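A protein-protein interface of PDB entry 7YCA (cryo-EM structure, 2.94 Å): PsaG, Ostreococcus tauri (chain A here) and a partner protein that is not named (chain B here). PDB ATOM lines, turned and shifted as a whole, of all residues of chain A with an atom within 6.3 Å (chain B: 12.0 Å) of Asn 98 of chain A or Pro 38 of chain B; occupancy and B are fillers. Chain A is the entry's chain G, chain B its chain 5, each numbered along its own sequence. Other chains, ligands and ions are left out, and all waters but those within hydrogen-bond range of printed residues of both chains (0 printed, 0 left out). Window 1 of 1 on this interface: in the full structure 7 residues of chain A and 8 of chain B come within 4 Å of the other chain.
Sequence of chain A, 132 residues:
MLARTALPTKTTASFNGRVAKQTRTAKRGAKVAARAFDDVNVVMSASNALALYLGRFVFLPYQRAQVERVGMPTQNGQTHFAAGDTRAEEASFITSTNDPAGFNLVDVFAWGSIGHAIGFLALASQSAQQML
The backbone carbonyl oxygen (O) of Gly 54 of chain B is in hydrogen-bond range of the side-chain hydroxyl (OH) of Tyr 39 of chain B (2.8 Å). The side-chain hydroxyl of Tyr 39 of chain B is in hydrogen-bond range of the indole nitrogen of Trp 34 of chain B (3.2 Å). The side-chain hydroxyl (OG1) of Thr 95 of chain A sits at hydrogen-bond distance from the backbone carbonyl oxygen (O) of Ser 92 of chain A (3.3 Å).
Among the printed residues, merely in contact across the chains: Ser 92 of chain A with Tyr 39 of chain B (3.7 Å), Ser 92 of chain A with Lys 40 of chain B (3.2 Å), Ser 92 of chain A with Pro 42 of chain B (3.6 Å), Ser 96 of chain A with Leu 35 of chain B (3.5 Å), Ser 96 of chain A with Pro 38 of chain B (3.6 Å), Ser 96 of chain A with Tyr 39 of chain B (3.6 Å) and Asn 98 of chain A with Pro 38 of chain B (3.7 Å).
Printed residues of chain B within 4 Å of Ser 92 of chain A: Tyr 39 (3.7 Å), Lys 40 (3.2 Å) and Pro 42 (3.6 Å). Thr 97 of chain A touches none of the printed residues of chain B. Of chain B, only Pro 38 comes within 4 Å of Asn 98 of chain A. No residue of chain B comes within 4 Å of Asp 99 of chain A. Ala 101 of chain A touches none of the printed residues of chain B. Of the printed residues of chain A, Leu 35 of chain B touches Ser 96. Pro 38 of chain B touches two residues of chain A. Of the printed residues of chain A, Tyr 39 of chain B touches Ser 92 and Ser 96. Of the printed residues of chain A, Lys 40 of chain B touches Ser 92. Ala 41 of chain B touches none of the printed residues of chain A. Printed residues of chain A within 4 Å of Pro 42 of chain B: Ser 92. The nearest printed residue of chain B that does not touch Ser 92 of chain A is Ala 41 of chain B (4.1 Å).
Of the 13 printed residues of chain B, 5 touch a printed residue of chain A. Printed residues of chain B that touch a printed residue of chain A: Leu 35, Pro 38, Tyr 39, Lys 40 and Pro 42. Hydrophobic or aromatic side chains of chain B within 4 Å of the printed part of chain A: Leu 35, Pro 38, Tyr 39 and Pro 42. Along chain B the printed residues that touch a printed residue of chain A span positions 35 to 42. Of the 9 printed residues of chain A, 3 touch a printed residue of chain B. Printed residues of chain A that touch a printed residue of chain B: Ser 92, Ser 96 and Asn 98. Among the printed residues, no Asp or Glu carboxylate lies within 4 Å of a Lys or Arg side-chain nitrogen of the other chain.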
ATOM      1  N   SER A  92       4.821   1.660  17.150  1.00  0.00           N
ATOM      2  CA  SER A  92       3.411   1.768  17.512  1.00  0.00           C
ATOM      3  C   SER A  92       2.597   0.521  17.178  1.00  0.00           C
ATOM      4  O   SER A  92       1.632   0.221  17.889  1.00  0.00           O
ATOM      5  CB  SER A  92       2.781   2.976  16.807  1.00  0.00           C
ATOM      6  OG  SER A  92       3.617   4.116  16.901  1.00  0.00           O
ATOM      7  N   THR A  95       1.638  -2.778  19.789  1.00  0.00           N
ATOM      8  CA  THR A  95       0.559  -2.858  20.763  1.00  0.00           C
ATOM      9  C   THR A  95      -0.819  -2.892  20.123  1.00  0.00           C
ATOM     10  O   THR A  95      -1.798  -3.155  20.829  1.00  0.00           O
ATOM     11  CB  THR A  95       0.637  -1.673  21.736  1.00  0.00           C
ATOM     12  OG1 THR A  95       0.718  -0.452  20.994  1.00  0.00           O
ATOM     13  CG2 THR A  95       1.861  -1.800  22.641  1.00  0.00           C
ATOM     14  N   SER A  96      -0.925  -2.659  18.814  1.00  0.00           N
ATOM     15  CA  SER A  96      -2.210  -2.645  18.122  1.00  0.00           C
ATOM     16  C   SER A  96      -2.649  -4.076  17.875  1.00  0.00           C
ATOM     17  O   SER A  96      -2.340  -4.678  16.845  1.00  0.00           O
ATOM     18  CB  SER A  96      -2.106  -1.881  16.814  1.00  0.00           C
ATOM     19  OG  SER A  96      -1.839  -2.757  15.739  1.00  0.00           O
ATOM     20  N   THR A  97      -3.342  -4.665  18.841  1.00  0.00           N
ATOM     21  CA  THR A  97      -3.726  -6.068  18.701  1.00  0.00           C
ATOM     22  C   THR A  97      -5.039  -6.374  19.403  1.00  0.00           C
ATOM     23  O   THR A  97      -5.258  -5.942  20.534  1.00  0.00           O
ATOM     24  CB  THR A  97      -2.631  -7.006  19.251  1.00  0.00           C
ATOM     25  OG1 THR A  97      -1.359  -6.632  18.707  1.00  0.00           O
ATOM     26  CG2 THR A  97      -2.929  -8.451  18.886  1.00  0.00           C
ATOM     27  N   ASN A  98      -5.913  -7.119  18.736  1.00  0.00           N
ATOM     28  CA  ASN A  98      -7.197  -7.473  19.330  1.00  0.00           C
ATOM     29  C   ASN A  98      -7.117  -8.813  20.042  1.00  0.00           C
ATOM     30  O   ASN A  98      -8.119  -9.310  20.554  1.00  0.00           O
ATOM     31  CB  ASN A  98      -8.286  -7.512  18.259  1.00  0.00           C
ATOM     32  CG  ASN A  98      -8.388  -6.214  17.486  1.00  0.00           C
ATOM     33  OD1 ASN A  98      -7.668  -5.253  17.760  1.00  0.00           O
ATOM     34  ND2 ASN A  98      -9.288  -6.177  16.509  1.00  0.00           N
ATOM     35  N   ASP A  99      -5.927  -9.403  20.074  1.00  0.00           N
ATOM     36  CA  ASP A  99      -5.752 -10.672  20.766  1.00  0.00           C
ATOM     37  C   ASP A  99      -6.074 -10.535  22.238  1.00  0.00           C
ATOM     38  O   ASP A  99      -5.643  -9.581  22.886  1.00  0.00           O
ATOM     39  CB  ASP A  99      -4.322 -11.179  20.609  1.00  0.00           C
ATOM     40  CG  ASP A  99      -4.187 -12.205  19.513  1.00  0.00           C
ATOM     41  OD1 ASP A  99      -5.078 -13.069  19.390  1.00  0.00           O
ATOM     42  OD2 ASP A  99      -3.179 -12.152  18.784  1.00  0.00           O
ATOM     43  N   PRO A 100      -6.832 -11.494  22.779  1.00  0.00           N
ATOM     44  CA  PRO A 100      -7.132 -11.468  24.212  1.00  0.00           C
ATOM     45  C   PRO A 100      -5.851 -11.452  25.030  1.00  0.00           C
ATOM     46  O   PRO A 100      -5.810 -10.816  26.083  1.00  0.00           O
ATOM     47  CB  PRO A 100      -7.881 -12.782  24.429  1.00  0.00           C
ATOM     48  CG  PRO A 100      -8.512 -13.077  23.109  1.00  0.00           C
ATOM     49  CD  PRO A 100      -7.570 -12.550  22.066  1.00  0.00           C
ATOM     50  N   ALA A 101      -4.817 -12.138  24.556  1.00  0.00           N
ATOM     51  CA  ALA A 101      -3.549 -12.192  25.279  1.00  0.00           C
ATOM     52  C   ALA A 101      -2.510 -11.250  24.683  1.00  0.00           C
ATOM     53  O   ALA A 101      -1.319 -11.378  24.968  1.00  0.00           O
ATOM     54  CB  ALA A 101      -3.020 -13.617  25.312  1.00  0.00           C
ATOM     55  N   GLY A 102      -2.950 -10.307  23.856  1.00  0.00           N
ATOM     56  CA  GLY A 102      -2.032  -9.341  23.276  1.00  0.00           C
ATOM     57  C   GLY A 102      -0.899  -9.953  22.482  1.00  0.00           C
ATOM     58  O   GLY A 102       0.255  -9.551  22.632  1.00  0.00           O
ATOM     59  N   LYS B  32      -7.834   4.173   6.725  1.00  0.00           N
ATOM     60  CA  LYS B  32      -7.098   5.338   7.205  1.00  0.00           C
ATOM     61  C   LYS B  32      -5.645   4.981   7.485  1.00  0.00           C
ATOM     62  O   LYS B  32      -4.742   5.747   7.151  1.00  0.00           O
ATOM     63  CB  LYS B  32      -7.752   5.902   8.472  1.00  0.00           C
ATOM     64  CG  LYS B  32      -7.152   7.219   8.978  1.00  0.00           C
ATOM     65  CD  LYS B  32      -7.763   7.632  10.300  1.00  0.00           C
ATOM     66  CE  LYS B  32      -7.191   8.955  10.772  1.00  0.00           C
ATOM     67  NZ  LYS B  32      -7.747   9.364  12.088  1.00  0.00           N
ATOM     68  N   MET B  33      -5.440   3.822   8.106  1.00  0.00           N
ATOM     69  CA  MET B  33      -4.141   3.380   8.592  1.00  0.00           C
ATOM     70  C   MET B  33      -3.813   2.022   8.001  1.00  0.00           C
ATOM     71  O   MET B  33      -4.705   1.210   7.762  1.00  0.00           O
ATOM     72  CB  MET B  33      -4.125   3.249  10.111  1.00  0.00           C
ATOM     73  CG  MET B  33      -4.409   4.521  10.869  1.00  0.00           C
ATOM     74  SD  MET B  33      -2.938   5.486  11.139  1.00  0.00           S
ATOM     75  CE  MET B  33      -3.582   6.659  12.325  1.00  0.00           C
ATOM     76  N   TRP B  34      -2.516   1.735   7.871  1.00  0.00           N
ATOM     77  CA  TRP B  34      -2.088   0.459   7.303  1.00  0.00           C
ATOM     78  C   TRP B  34      -2.459  -0.752   8.159  1.00  0.00           C
ATOM     79  O   TRP B  34      -2.313  -1.879   7.674  1.00  0.00           O
ATOM     80  CB  TRP B  34      -0.575   0.455   7.065  1.00  0.00           C
ATOM     81  CG  TRP B  34       0.270   0.477   8.302  1.00  0.00           C
ATOM     82  CD1 TRP B  34       0.489   1.542   9.119  1.00  0.00           C
ATOM     83  CD2 TRP B  34       1.024  -0.610   8.856  1.00  0.00           C
ATOM     84  NE1 TRP B  34       1.328   1.193  10.140  1.00  0.00           N
ATOM     85  CE2 TRP B  34       1.673  -0.123  10.006  1.00  0.00           C
ATOM     86  CE3 TRP B  34       1.232  -1.939   8.479  1.00  0.00           C
ATOM     87  CZ2 TRP B  34       2.503  -0.916  10.788  1.00  0.00           C
ATOM     88  CZ3 TRP B  34       2.050  -2.730   9.265  1.00  0.00           C
ATOM     89  CH2 TRP B  34       2.677  -2.216  10.404  1.00  0.00           C
ATOM     90  N   LEU B  35      -2.912  -0.556   9.393  1.00  0.00           N
ATOM     91  CA  LEU B  35      -3.350  -1.601  10.304  1.00  0.00           C
ATOM     92  C   LEU B  35      -4.756  -1.289  10.787  1.00  0.00           C
ATOM     93  O   LEU B  35      -5.232  -0.158  10.632  1.00  0.00           O
ATOM     94  CB  LEU B  35      -2.377  -1.701  11.489  1.00  0.00           C
ATOM     95  CG  LEU B  35      -1.127  -2.571  11.306  1.00  0.00           C
ATOM     96  CD1 LEU B  35      -0.317  -2.582  12.574  1.00  0.00           C
ATOM     97  CD2 LEU B  35      -1.394  -4.015  10.860  1.00  0.00           C
ATOM     98  N   PRO B  36      -5.472  -2.284  11.371  1.00  0.00           N
ATOM     99  CA  PRO B  36      -6.880  -2.047  11.727  1.00  0.00           C
ATOM    100  C   PRO B  36      -7.060  -1.002  12.823  1.00  0.00           C
ATOM    101  O   PRO B  36      -6.071  -0.455  13.323  1.00  0.00           O
ATOM    102  CB  PRO B  36      -7.368  -3.436  12.166  1.00  0.00           C
ATOM    103  CG  PRO B  36      -6.150  -4.167  12.554  1.00  0.00           C
ATOM    104  CD  PRO B  36      -5.086  -3.686  11.634  1.00  0.00           C
ATOM    105  N   ALA B  37      -8.320  -0.745  13.197  1.00  0.00           N
ATOM    106  CA  ALA B  37      -8.689   0.512  13.853  1.00  0.00           C
ATOM    107  C   ALA B  37      -7.942   0.798  15.156  1.00  0.00           C
ATOM    108  O   ALA B  37      -7.573   1.968  15.369  1.00  0.00           O
ATOM    109  CB  ALA B  37     -10.208   0.546  14.075  1.00  0.00           C
ATOM    110  N   PRO B  38      -7.646  -0.202  16.050  1.00  0.00           N
ATOM    111  CA  PRO B  38      -6.822   0.090  17.234  1.00  0.00           C
ATOM    112  C   PRO B  38      -5.326   0.266  16.993  1.00  0.00           C
ATOM    113  O   PRO B  38      -4.600   0.449  17.966  1.00  0.00           O
ATOM    114  CB  PRO B  38      -7.077  -1.093  18.154  1.00  0.00           C
ATOM    115  CG  PRO B  38      -8.313  -1.636  17.708  1.00  0.00           C
ATOM    116  CD  PRO B  38      -8.273  -1.512  16.218  1.00  0.00           C
ATOM    117  N   TYR B  39      -4.910   0.488  15.743  1.00  0.00           N
ATOM    118  CA  TYR B  39      -3.587   1.039  15.435  1.00  0.00           C
ATOM    119  C   TYR B  39      -3.520   2.569  15.435  1.00  0.00           C
ATOM    120  O   TYR B  39      -4.338   3.231  14.788  1.00  0.00           O
ATOM    121  CB  TYR B  39      -3.140   0.570  14.066  1.00  0.00           C
ATOM    122  CG  TYR B  39      -1.802   1.146  13.728  1.00  0.00           C
ATOM    123  CD1 TYR B  39      -0.680   0.774  14.443  1.00  0.00           C
ATOM    124  CD2 TYR B  39      -1.661   2.084  12.721  1.00  0.00           C
ATOM    125  CE1 TYR B  39       0.543   1.304  14.163  1.00  0.00           C
ATOM    126  CE2 TYR B  39      -0.438   2.623  12.429  1.00  0.00           C
ATOM    127  CZ  TYR B  39       0.661   2.233  13.160  1.00  0.00           C
ATOM    128  OH  TYR B  39       1.892   2.761  12.861  1.00  0.00           O
ATOM    129  N   LYS B  40      -2.563   3.124  16.190  1.00  0.00           N
ATOM    130  CA  LYS B  40      -2.396   4.568  16.370  1.00  0.00           C
ATOM    131  C   LYS B  40      -1.075   4.947  15.718  1.00  0.00           C
ATOM    132  O   LYS B  40      -0.040   4.341  16.024  1.00  0.00           O
ATOM    133  CB  LYS B  40      -2.377   4.990  17.860  1.00  0.00           C
ATOM    134  N   ALA B  41      -1.100   5.936  14.825  1.00  0.00           N
ATOM    135  CA  ALA B  41       0.094   6.224  14.052  1.00  0.00           C
ATOM    136  C   ALA B  41       1.178   6.817  14.945  1.00  0.00           C
ATOM    137  O   ALA B  41       0.877   7.425  15.976  1.00  0.00           O
ATOM    138  CB  ALA B  41      -0.171   7.205  12.919  1.00  0.00           C
ATOM    139  N   PRO B  42       2.445   6.681  14.564  1.00  0.00           N
ATOM    140  CA  PRO B  42       3.490   7.386  15.302  1.00  0.00           C
ATOM    141  C   PRO B  42       3.361   8.890  15.116  1.00  0.00           C
ATOM    142  O   PRO B  42       2.698   9.378  14.197  1.00  0.00           O
ATOM    143  CB  PRO B  42       4.781   6.852  14.688  1.00  0.00           C
ATOM    144  CG  PRO B  42       4.393   6.374  13.329  1.00  0.00           C
ATOM    145  CD  PRO B  42       3.013   5.859  13.477  1.00  0.00           C
ATOM    146  N   TYR B  53      -0.692   6.831   5.693  1.00  0.00           N
ATOM    147  CA  TYR B  53      -1.387   5.783   6.425  1.00  0.00           C
ATOM    148  C   TYR B  53      -0.638   5.368   7.690  1.00  0.00           C
ATOM    149  O   TYR B  53      -0.920   4.307   8.249  1.00  0.00           O
ATOM    150  CB  TYR B  53      -1.610   4.594   5.497  1.00  0.00           C
ATOM    151  CG  TYR B  53      -2.289   4.991   4.199  1.00  0.00           C
ATOM    152  CD1 TYR B  53      -3.651   5.236   4.150  1.00  0.00           C
ATOM    153  CD2 TYR B  53      -1.558   5.150   3.031  1.00  0.00           C
ATOM    154  CE1 TYR B  53      -4.269   5.604   2.968  1.00  0.00           C
ATOM    155  CE2 TYR B  53      -2.161   5.522   1.846  1.00  0.00           C
ATOM    156  CZ  TYR B  53      -3.517   5.741   1.818  1.00  0.00           C
ATOM    157  OH  TYR B  53      -4.119   6.105   0.637  1.00  0.00           O
ATOM    158  N   GLY B  54       0.296   6.192   8.161  1.00  0.00           N
ATOM    159  CA  GLY B  54       1.010   5.903   9.394  1.00  0.00           C
ATOM    160  C   GLY B  54       1.878   4.664   9.343  1.00  0.00           C
ATOM    161  O   GLY B  54       1.991   3.955  10.351  1.00  0.00           O
